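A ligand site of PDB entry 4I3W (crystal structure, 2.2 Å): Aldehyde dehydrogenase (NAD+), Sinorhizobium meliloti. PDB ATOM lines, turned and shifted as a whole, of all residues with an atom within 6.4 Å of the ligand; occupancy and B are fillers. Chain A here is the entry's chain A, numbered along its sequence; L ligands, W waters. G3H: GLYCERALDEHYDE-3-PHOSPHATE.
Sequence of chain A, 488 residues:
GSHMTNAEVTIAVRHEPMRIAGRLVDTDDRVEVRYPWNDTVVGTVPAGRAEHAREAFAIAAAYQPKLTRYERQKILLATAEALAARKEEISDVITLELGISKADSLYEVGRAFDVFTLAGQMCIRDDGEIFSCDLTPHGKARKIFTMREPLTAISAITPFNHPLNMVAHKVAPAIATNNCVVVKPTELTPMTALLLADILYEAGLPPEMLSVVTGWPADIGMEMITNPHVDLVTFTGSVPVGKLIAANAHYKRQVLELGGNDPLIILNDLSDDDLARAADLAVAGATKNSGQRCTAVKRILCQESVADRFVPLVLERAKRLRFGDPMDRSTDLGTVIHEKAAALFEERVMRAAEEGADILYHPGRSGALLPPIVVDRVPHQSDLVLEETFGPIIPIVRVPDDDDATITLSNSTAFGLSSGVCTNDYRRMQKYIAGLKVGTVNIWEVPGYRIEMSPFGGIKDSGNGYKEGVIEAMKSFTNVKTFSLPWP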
ATOM      1  N   ARG A 111      35.667 -17.839   3.265  1.00  0.00           N
ATOM      2  CA  ARG A 111      34.651 -16.793   3.182  1.00  0.00           C
ATOM      3  C   ARG A 111      35.073 -15.554   4.012  1.00  0.00           C
ATOM      4  O   ARG A 111      34.897 -14.424   3.578  1.00  0.00           O
ATOM      5  CB  ARG A 111      33.271 -17.307   3.634  1.00  0.00           C
ATOM      6  CG  ARG A 111      32.615 -18.320   2.635  1.00  0.00           C
ATOM      7  CD  ARG A 111      31.148 -18.581   3.023  1.00  0.00           C
ATOM      8  NE  ARG A 111      30.349 -17.339   2.981  1.00  0.00           N
ATOM      9  CZ  ARG A 111      29.177 -17.185   3.574  1.00  0.00           C
ATOM     10  NH1 ARG A 111      28.641 -18.209   4.237  1.00  0.00           N
ATOM     11  NH2 ARG A 111      28.531 -16.014   3.485  1.00  0.00           N
ATOM     12  N   PRO A 159      25.616 -15.764  15.945  1.00  0.00           N
ATOM     13  CA  PRO A 159      25.094 -17.094  16.209  1.00  0.00           C
ATOM     14  C   PRO A 159      26.160 -18.164  16.081  1.00  0.00           C
ATOM     15  O   PRO A 159      27.334 -17.858  15.728  1.00  0.00           O
ATOM     16  CB  PRO A 159      24.069 -17.257  15.115  1.00  0.00           C
ATOM     17  CG  PRO A 159      24.696 -16.570  13.938  1.00  0.00           C
ATOM     18  CD  PRO A 159      25.545 -15.434  14.517  1.00  0.00           C
ATOM     19  N   ASN A 161      26.369 -20.799  13.964  1.00  0.00           N
ATOM     20  CA  ASN A 161      26.572 -21.544  12.712  1.00  0.00           C
ATOM     21  C   ASN A 161      27.728 -21.094  11.849  1.00  0.00           C
ATOM     22  O   ASN A 161      28.215 -21.865  11.021  1.00  0.00           O
ATOM     23  CB  ASN A 161      25.268 -21.638  11.895  1.00  0.00           C
ATOM     24  CG  ASN A 161      24.874 -20.290  11.269  1.00  0.00           C
ATOM     25  OD1 ASN A 161      24.914 -19.245  11.917  1.00  0.00           O
ATOM     26  ND2 ASN A 161      24.498 -20.306   9.998  1.00  0.00           N
ATOM     27  N   HIS A 162      28.154 -19.835  12.002  1.00  0.00           N
ATOM     28  CA  HIS A 162      29.426 -19.399  11.364  1.00  0.00           C
ATOM     29  C   HIS A 162      30.247 -18.618  12.371  1.00  0.00           C
ATOM     30  O   HIS A 162      30.220 -17.368  12.353  1.00  0.00           O
ATOM     31  CB  HIS A 162      29.226 -18.527  10.107  1.00  0.00           C
ATOM     32  CG  HIS A 162      28.441 -19.180   9.014  1.00  0.00           C
ATOM     33  ND1 HIS A 162      28.858 -20.348   8.384  1.00  0.00           N
ATOM     34  CD2 HIS A 162      27.296 -18.810   8.391  1.00  0.00           C
ATOM     35  CE1 HIS A 162      27.984 -20.675   7.454  1.00  0.00           C
ATOM     36  NE2 HIS A 162      27.015 -19.763   7.440  1.00  0.00           N
ATOM     37  N   ASN A 165      32.800 -16.388  10.237  1.00  0.00           N
ATOM     38  CA  ASN A 165      32.264 -15.517   9.179  1.00  0.00           C
ATOM     39  C   ASN A 165      31.166 -14.544   9.625  1.00  0.00           C
ATOM     40  O   ASN A 165      31.078 -13.438   9.096  1.00  0.00           O
ATOM     41  CB  ASN A 165      31.765 -16.315   7.982  1.00  0.00           C
ATOM     42  CG  ASN A 165      31.894 -15.535   6.706  1.00  0.00           C
ATOM     43  OD1 ASN A 165      32.930 -14.914   6.485  1.00  0.00           O
ATOM     44  ND2 ASN A 165      30.843 -15.537   5.852  1.00  0.00           N
ATOM     45  N   MET A 166      30.345 -14.937  10.585  1.00  0.00           N
ATOM     46  CA  MET A 166      29.329 -14.007  11.090  1.00  0.00           C
ATOM     47  C   MET A 166      29.953 -12.858  11.877  1.00  0.00           C
ATOM     48  O   MET A 166      29.431 -11.734  11.892  1.00  0.00           O
ATOM     49  CB  MET A 166      28.305 -14.714  11.948  1.00  0.00           C
ATOM     50  CG  MET A 166      27.421 -15.622  11.147  1.00  0.00           C
ATOM     51  SD  MET A 166      26.040 -14.695  10.474  1.00  0.00           S
ATOM     52  CE  MET A 166      26.706 -13.919   8.987  1.00  0.00           C
ATOM     53  N   HIS A 169      31.553 -10.553   9.068  1.00  0.00           N
ATOM     54  CA  HIS A 169      30.532  -9.694   8.415  1.00  0.00           C
ATOM     55  C   HIS A 169      30.053  -8.516   9.279  1.00  0.00           C
ATOM     56  O   HIS A 169      29.623  -7.518   8.743  1.00  0.00           O
ATOM     57  CB  HIS A 169      29.317 -10.518   7.990  1.00  0.00           C
ATOM     58  CG  HIS A 169      29.400 -11.036   6.598  1.00  0.00           C
ATOM     59  ND1 HIS A 169      29.227 -10.225   5.495  1.00  0.00           N
ATOM     60  CD2 HIS A 169      29.603 -12.297   6.120  1.00  0.00           C
ATOM     61  CE1 HIS A 169      29.345 -10.947   4.393  1.00  0.00           C
ATOM     62  NE2 HIS A 169      29.567 -12.214   4.743  1.00  0.00           N
ATOM     63  N   THR A 236      22.247 -11.684  14.278  1.00  0.00           N
ATOM     64  CA  THR A 236      21.884 -12.797  13.443  1.00  0.00           C
ATOM     65  C   THR A 236      21.638 -13.955  14.382  1.00  0.00           C
ATOM     66  O   THR A 236      22.463 -14.233  15.259  1.00  0.00           O
ATOM     67  CB  THR A 236      23.034 -13.147  12.488  1.00  0.00           C
ATOM     68  OG1 THR A 236      23.328 -12.024  11.658  1.00  0.00           O
ATOM     69  CG2 THR A 236      22.678 -14.331  11.607  1.00  0.00           C
ATOM     70  N   GLU A 257      18.759 -10.395  11.264  1.00  0.00           N
ATOM     71  CA  GLU A 257      18.619 -11.479  10.306  1.00  0.00           C
ATOM     72  C   GLU A 257      18.293 -12.702  11.125  1.00  0.00           C
ATOM     73  O   GLU A 257      19.028 -13.097  12.057  1.00  0.00           O
ATOM     74  CB  GLU A 257      19.876 -11.719   9.448  1.00  0.00           C
ATOM     75  CG  GLU A 257      20.177 -10.596   8.471  1.00  0.00           C
ATOM     76  CD  GLU A 257      19.002 -10.248   7.555  1.00  0.00           C
ATOM     77  OE1 GLU A 257      18.167 -11.156   7.220  1.00  0.00           O
ATOM     78  OE2 GLU A 257      18.937  -9.054   7.150  1.00  0.00           O
ATOM     79  N   LEU A 258      17.142 -13.243  10.805  1.00  0.00           N
ATOM     80  CA  LEU A 258      16.614 -14.346  11.541  1.00  0.00           C
ATOM     81  C   LEU A 258      16.729 -15.533  10.594  1.00  0.00           C
ATOM     82  O   LEU A 258      17.476 -15.489   9.609  1.00  0.00           O
ATOM     83  CB  LEU A 258      15.197 -14.010  11.961  1.00  0.00           C
ATOM     84  CG  LEU A 258      15.006 -12.981  13.091  1.00  0.00           C
ATOM     85  CD1 LEU A 258      16.239 -12.147  13.424  1.00  0.00           C
ATOM     86  CD2 LEU A 258      13.807 -12.042  12.857  1.00  0.00           C
ATOM     87  N   ASN A 289      27.832 -27.333   5.630  1.00  0.00           N
ATOM     88  CA  ASN A 289      27.790 -26.811   6.973  1.00  0.00           C
ATOM     89  C   ASN A 289      26.811 -27.592   7.863  1.00  0.00           C
ATOM     90  O   ASN A 289      26.194 -27.053   8.813  1.00  0.00           O
ATOM     91  CB  ASN A 289      27.457 -25.307   6.953  1.00  0.00           C
ATOM     92  CG  ASN A 289      28.129 -24.560   8.099  1.00  0.00           C
ATOM     93  OD1 ASN A 289      29.332 -24.707   8.312  1.00  0.00           O
ATOM     94  ND2 ASN A 289      27.337 -23.803   8.886  1.00  0.00           N
ATOM     95  N   GLN A 292      23.534 -26.198   8.463  1.00  0.00           N
ATOM     96  CA  GLN A 292      23.336 -25.093   9.420  1.00  0.00           C
ATOM     97  C   GLN A 292      23.597 -23.751   8.780  1.00  0.00           C
ATOM     98  O   GLN A 292      24.591 -23.065   9.090  1.00  0.00           O
ATOM     99  CB  GLN A 292      24.172 -25.312  10.689  1.00  0.00           C
ATOM    100  CG  GLN A 292      23.721 -26.560  11.468  1.00  0.00           C
ATOM    101  CD  GLN A 292      24.682 -26.999  12.573  1.00  0.00           C
ATOM    102  OE1 GLN A 292      24.276 -27.236  13.674  1.00  0.00           O
ATOM    103  NE2 GLN A 292      25.929 -27.130  12.278  1.00  0.00           N
ATOM    104  N   ARG A 293      22.710 -23.404   7.861  1.00  0.00           N
ATOM    105  CA  ARG A 293      22.727 -22.113   7.171  1.00  0.00           C
ATOM    106  C   ARG A 293      21.303 -21.554   7.149  1.00  0.00           C
ATOM    107  O   ARG A 293      20.352 -22.304   6.930  1.00  0.00           O
ATOM    108  CB  ARG A 293      23.194 -22.260   5.719  1.00  0.00           C
ATOM    109  CG  ARG A 293      24.658 -22.498   5.537  1.00  0.00           C
ATOM    110  CD  ARG A 293      25.059 -22.416   4.071  1.00  0.00           C
ATOM    111  NE  ARG A 293      25.253 -21.027   3.620  1.00  0.00           N
ATOM    112  CZ  ARG A 293      25.558 -20.694   2.376  1.00  0.00           C
ATOM    113  NH1 ARG A 293      25.649 -21.633   1.436  1.00  0.00           N
ATOM    114  NH2 ARG A 293      25.733 -19.435   2.062  1.00  0.00           N
ATOM    115  N   CYS A 294      21.157 -20.257   7.348  1.00  0.00           N
ATOM    116  CA  CYS A 294      19.850 -19.635   7.270  1.00  0.00           C
ATOM    117  C   CYS A 294      19.293 -19.889   5.872  1.00  0.00           C
ATOM    118  O   CYS A 294      18.079 -19.973   5.723  1.00  0.00           O
ATOM    119  CB  CYS A 294      19.935 -18.150   7.548  1.00  0.00           C
ATOM    120  SG  CYS A 294      21.200 -17.322   6.584  1.00  0.00           S
ATOM    121  N   THR A 295      20.187 -20.006   4.883  1.00  0.00           N
ATOM    122  CA  THR A 295      19.819 -20.193   3.464  1.00  0.00           C
ATOM    123  C   THR A 295      20.070 -21.639   2.973  1.00  0.00           C
ATOM    124  O   THR A 295      20.129 -21.891   1.759  1.00  0.00           O
ATOM    125  CB  THR A 295      20.592 -19.256   2.564  1.00  0.00           C
ATOM    126  OG1 THR A 295      21.992 -19.354   2.884  1.00  0.00           O
ATOM    127  CG2 THR A 295      20.126 -17.797   2.737  1.00  0.00           C
ATOM    128  N   ALA A 296      20.264 -22.571   3.892  1.00  0.00           N
ATOM    129  CA  ALA A 296      20.344 -23.987   3.513  1.00  0.00           C
ATOM    130  C   ALA A 296      19.114 -24.386   2.706  1.00  0.00           C
ATOM    131  O   ALA A 296      18.001 -23.844   2.905  1.00  0.00           O
ATOM    132  CB  ALA A 296      20.447 -24.873   4.760  1.00  0.00           C
ATOM    133  N   PHE A 390      17.279 -27.186  11.071  1.00  0.00           N
ATOM    134  CA  PHE A 390      18.631 -26.651  10.910  1.00  0.00           C
ATOM    135  C   PHE A 390      19.688 -27.775  10.897  1.00  0.00           C
ATOM    136  O   PHE A 390      20.691 -27.694  11.588  1.00  0.00           O
ATOM    137  CB  PHE A 390      18.939 -25.686  12.066  1.00  0.00           C
ATOM    138  CG  PHE A 390      19.782 -24.516  11.688  1.00  0.00           C
ATOM    139  CD1 PHE A 390      19.417 -23.676  10.633  1.00  0.00           C
ATOM    140  CD2 PHE A 390      20.920 -24.206  12.426  1.00  0.00           C
ATOM    141  CE1 PHE A 390      20.204 -22.577  10.294  1.00  0.00           C
ATOM    142  CE2 PHE A 390      21.732 -23.092  12.099  1.00  0.00           C
ATOM    143  CZ  PHE A 390      21.370 -22.278  11.030  1.00  0.00           C
ATOM    144  N   LEU A 417      13.652 -15.691   2.767  1.00  0.00           N
ATOM    145  CA  LEU A 417      15.016 -15.266   2.743  1.00  0.00           C
ATOM    146  C   LEU A 417      15.553 -15.462   1.332  1.00  0.00           C
ATOM    147  O   LEU A 417      15.563 -14.521   0.525  1.00  0.00           O
ATOM    148  CB  LEU A 417      15.814 -15.989   3.827  1.00  0.00           C
ATOM    149  CG  LEU A 417      17.299 -15.602   3.990  1.00  0.00           C
ATOM    150  CD1 LEU A 417      17.398 -14.155   4.279  1.00  0.00           C
ATOM    151  CD2 LEU A 417      17.914 -16.413   5.093  1.00  0.00           C
ATOM    152  N   GLY A 448      21.669 -20.585  -1.018  1.00  0.00           N
ATOM    153  CA  GLY A 448      22.726 -20.050  -0.189  1.00  0.00           C
ATOM    154  C   GLY A 448      23.753 -19.266  -0.984  1.00  0.00           C
ATOM    155  O   GLY A 448      24.608 -18.585  -0.425  1.00  0.00           O
ATOM    156  N   TYR A 449      23.700 -19.375  -2.302  1.00  0.00           N
ATOM    157  CA  TYR A 449      24.700 -18.695  -3.090  1.00  0.00           C
ATOM    158  C   TYR A 449      24.564 -17.153  -3.037  1.00  0.00           C
ATOM    159  O   TYR A 449      23.471 -16.603  -3.284  1.00  0.00           O
ATOM    160  CB  TYR A 449      24.749 -19.167  -4.560  1.00  0.00           C
ATOM    161  CG  TYR A 449      25.822 -18.385  -5.272  1.00  0.00           C
ATOM    162  CD1 TYR A 449      27.170 -18.738  -5.124  1.00  0.00           C
ATOM    163  CD2 TYR A 449      25.524 -17.213  -5.970  1.00  0.00           C
ATOM    164  CE1 TYR A 449      28.180 -17.991  -5.701  1.00  0.00           C
ATOM    165  CE2 TYR A 449      26.545 -16.454  -6.570  1.00  0.00           C
ATOM    166  CZ  TYR A 449      27.868 -16.850  -6.424  1.00  0.00           C
ATOM    167  OH  TYR A 449      28.922 -16.158  -6.975  1.00  0.00           O
ATOM    168  N   ARG A 450      25.664 -16.488  -2.697  1.00  0.00           N
ATOM    169  CA  ARG A 450      25.800 -15.027  -2.806  1.00  0.00           C
ATOM    170  C   ARG A 450      27.277 -14.701  -2.842  1.00  0.00           C
ATOM    171  O   ARG A 450      28.086 -15.578  -2.559  1.00  0.00           O
ATOM    172  CB  ARG A 450      25.161 -14.329  -1.624  1.00  0.00           C
ATOM    173  CG  ARG A 450      25.709 -14.769  -0.233  1.00  0.00           C
ATOM    174  CD  ARG A 450      25.153 -13.852   0.850  1.00  0.00           C
ATOM    175  NE  ARG A 450      25.401 -14.278   2.219  1.00  0.00           N
ATOM    176  CZ  ARG A 450      25.806 -13.456   3.190  1.00  0.00           C
ATOM    177  NH1 ARG A 450      26.040 -12.163   2.943  1.00  0.00           N
ATOM    178  NH2 ARG A 450      25.974 -13.911   4.426  1.00  0.00           N
ATOM    179  N   GLU A 452      30.117 -11.995  -1.015  1.00  0.00           N
ATOM    180  CA  GLU A 452      30.091 -11.441   0.328  1.00  0.00           C
ATOM    181  C   GLU A 452      29.725  -9.950   0.328  1.00  0.00           C
ATOM    182  O   GLU A 452      29.472  -9.361   1.386  1.00  0.00           O
ATOM    183  CB  GLU A 452      31.407 -11.672   1.069  1.00  0.00           C
ATOM    184  CG  GLU A 452      31.921 -13.106   1.022  1.00  0.00           C
ATOM    185  CD  GLU A 452      31.083 -14.128   1.807  1.00  0.00           C
ATOM    186  OE1 GLU A 452      30.192 -13.752   2.601  1.00  0.00           O
ATOM    187  OE2 GLU A 452      31.319 -15.337   1.587  1.00  0.00           O
ATOM    188  N   PHE A 456      22.091  -8.574   0.978  1.00  0.00           N
ATOM    189  CA  PHE A 456      21.603  -9.808   1.562  1.00  0.00           C
ATOM    190  C   PHE A 456      20.653  -9.498   2.670  1.00  0.00           C
ATOM    191  O   PHE A 456      20.977  -8.693   3.566  1.00  0.00           O
ATOM    192  CB  PHE A 456      22.725 -10.643   2.136  1.00  0.00           C
ATOM    193  CG  PHE A 456      22.241 -11.861   2.881  1.00  0.00           C
ATOM    194  CD1 PHE A 456      21.876 -13.024   2.203  1.00  0.00           C
ATOM    195  CD2 PHE A 456      22.141 -11.845   4.267  1.00  0.00           C
ATOM    196  CE1 PHE A 456      21.434 -14.150   2.906  1.00  0.00           C
ATOM    197  CE2 PHE A 456      21.691 -12.955   4.958  1.00  0.00           C
ATOM    198  CZ  PHE A 456      21.334 -14.097   4.278  1.00  0.00           C
ATOM    199  N   GLU A 468      22.147  -6.516   4.316  1.00  0.00           N
ATOM    200  CA  GLU A 468      23.455  -6.784   4.927  1.00  0.00           C
ATOM    201  C   GLU A 468      24.373  -7.131   3.746  1.00  0.00           C
ATOM    202  O   GLU A 468      24.044  -6.877   2.574  1.00  0.00           O
ATOM    203  CB  GLU A 468      23.369  -8.061   5.804  1.00  0.00           C
ATOM    204  CG  GLU A 468      23.435  -7.903   7.316  1.00  0.00           C
ATOM    205  CD  GLU A 468      23.796  -9.233   7.989  1.00  0.00           C
ATOM    206  OE1 GLU A 468      23.314 -10.268   7.513  1.00  0.00           O
ATOM    207  OE2 GLU A 468      24.607  -9.265   8.956  1.00  0.00           O
HETATM  208  O1  G3H L   1      23.477 -18.325   7.575  1.00  0.00           O
HETATM  209  C1  G3H L   1      22.741 -17.314   7.572  1.00  0.00           C
HETATM  210  C2  G3H L   1      23.425 -15.994   7.868  1.00  0.00           C
HETATM  211  O2  G3H L   1      22.505 -14.885   7.956  1.00  0.00           O
HETATM  212  C3  G3H L   1      24.335 -15.785   6.694  1.00  0.00           C
HETATM  213  O1P G3H L   1      23.987 -16.753   5.702  1.00  0.00           O
HETATM  214  O2P G3H L   1      25.031 -18.961   5.518  1.00  0.00           O
HETATM  215  O3P G3H L   1      24.882 -17.390   3.494  1.00  0.00           O
HETATM  216  O4P G3H L   1      26.447 -16.801   5.404  1.00  0.00           O
HETATM  217  P   G3H L   1      25.185 -17.526   4.960  1.00  0.00           P
HETATM  218  O   HOH W   1      28.357 -15.665   7.213  1.00  0.00           O
HETATM  219  O   HOH W   2      23.635 -12.251   9.172  1.00  0.00           O
HETATM  220  O   HOH W   3      19.148 -14.349   7.925  1.00  0.00           O
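An oxygen (O1) of the ligand sits at hydrogen-bond distance from the backbone NH (N) of Cys 294.
SG of Cys 294 is bonded to C1 of the ligand, at 1.8 Å.
NH2 of Arg 293 lies within salt-bridge range of O3P of the ligand (2.6 Å).
The guanidinium group (NH1) of Arg 111 lies within salt-bridge range of an oxygen (O4P) of the ligand (2.9 Å).
A ring nitrogen (NE2) of His 162 lies within hydrogen-bond range of an oxygen (O2P) of the ligand, 2.9 Å away.
The guanidinium group (NH2) of Arg 450 is in salt-bridge range of an oxygen (O4P) of the ligand (3.1 Å).
The side-chain amide nitrogen (ND2) of Asn 161 is in hydrogen-bond range of an oxygen (O1) of the ligand (3.3 Å).
The backbone carbonyl oxygen (O) of Gly 448 lies within hydrogen-bond range of the guanidinium group (NH2) of Arg 293 (2.9 Å).
The guanidinium group (NH2) of Arg 111 sits close to the side-chain amide nitrogen (ND2) of Asn 165, 3.3 Å away.
NE of Arg 111 lies within salt-bridge range of OE2 of Glu 452.
The side-chain amide nitrogen (ND2) of Asn 161 sits at hydrogen-bond distance from the backbone carbonyl oxygen (O) of Gln 292 (2.9 Å).
O of Asn 161 sits at hydrogen-bond distance from ND2 of Asn 289, 3.0 Å away.
N of Gly 448 sits at hydrogen-bond distance from O of Thr 295.
The backbone carbonyl oxygen of Phe 456 sits at hydrogen-bond distance from the backbone NH of Glu 468 (2.6 Å).
Residues that only touch the ligand: Met 166, Thr 236, Thr 295 and Phe 456.
Hydrophobic or aromatic side chains that line the ligand: His 162, Met 166 and Phe 456.
Of the 24 residues printed, 10 come within 4 Å of the ligand.
The nearest printed residue that does not touch the ligand is Gly 448 (4.1 Å).
Water W1 lies within hydrogen-bond range of the side-chain amide nitrogen (ND2) of Asn 165 (2.8 Å) and an oxygen (O4P) of the ligand (2.9 Å).
Water W2 lies within hydrogen-bond range of the side-chain hydroxyl of Thr 236 (2.5 Å), the side-chain carboxylate of Glu 468 (2.6 Å), an oxygen (O2) of the ligand (3.1 Å) and the side-chain sulfur of Met 166 (3.7 Å).
Water W3 lies within hydrogen-bond range of the backbone carbonyl oxygen of Leu 258, an oxygen (O2) of the ligand and the side-chain carboxylate of Glu 257.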
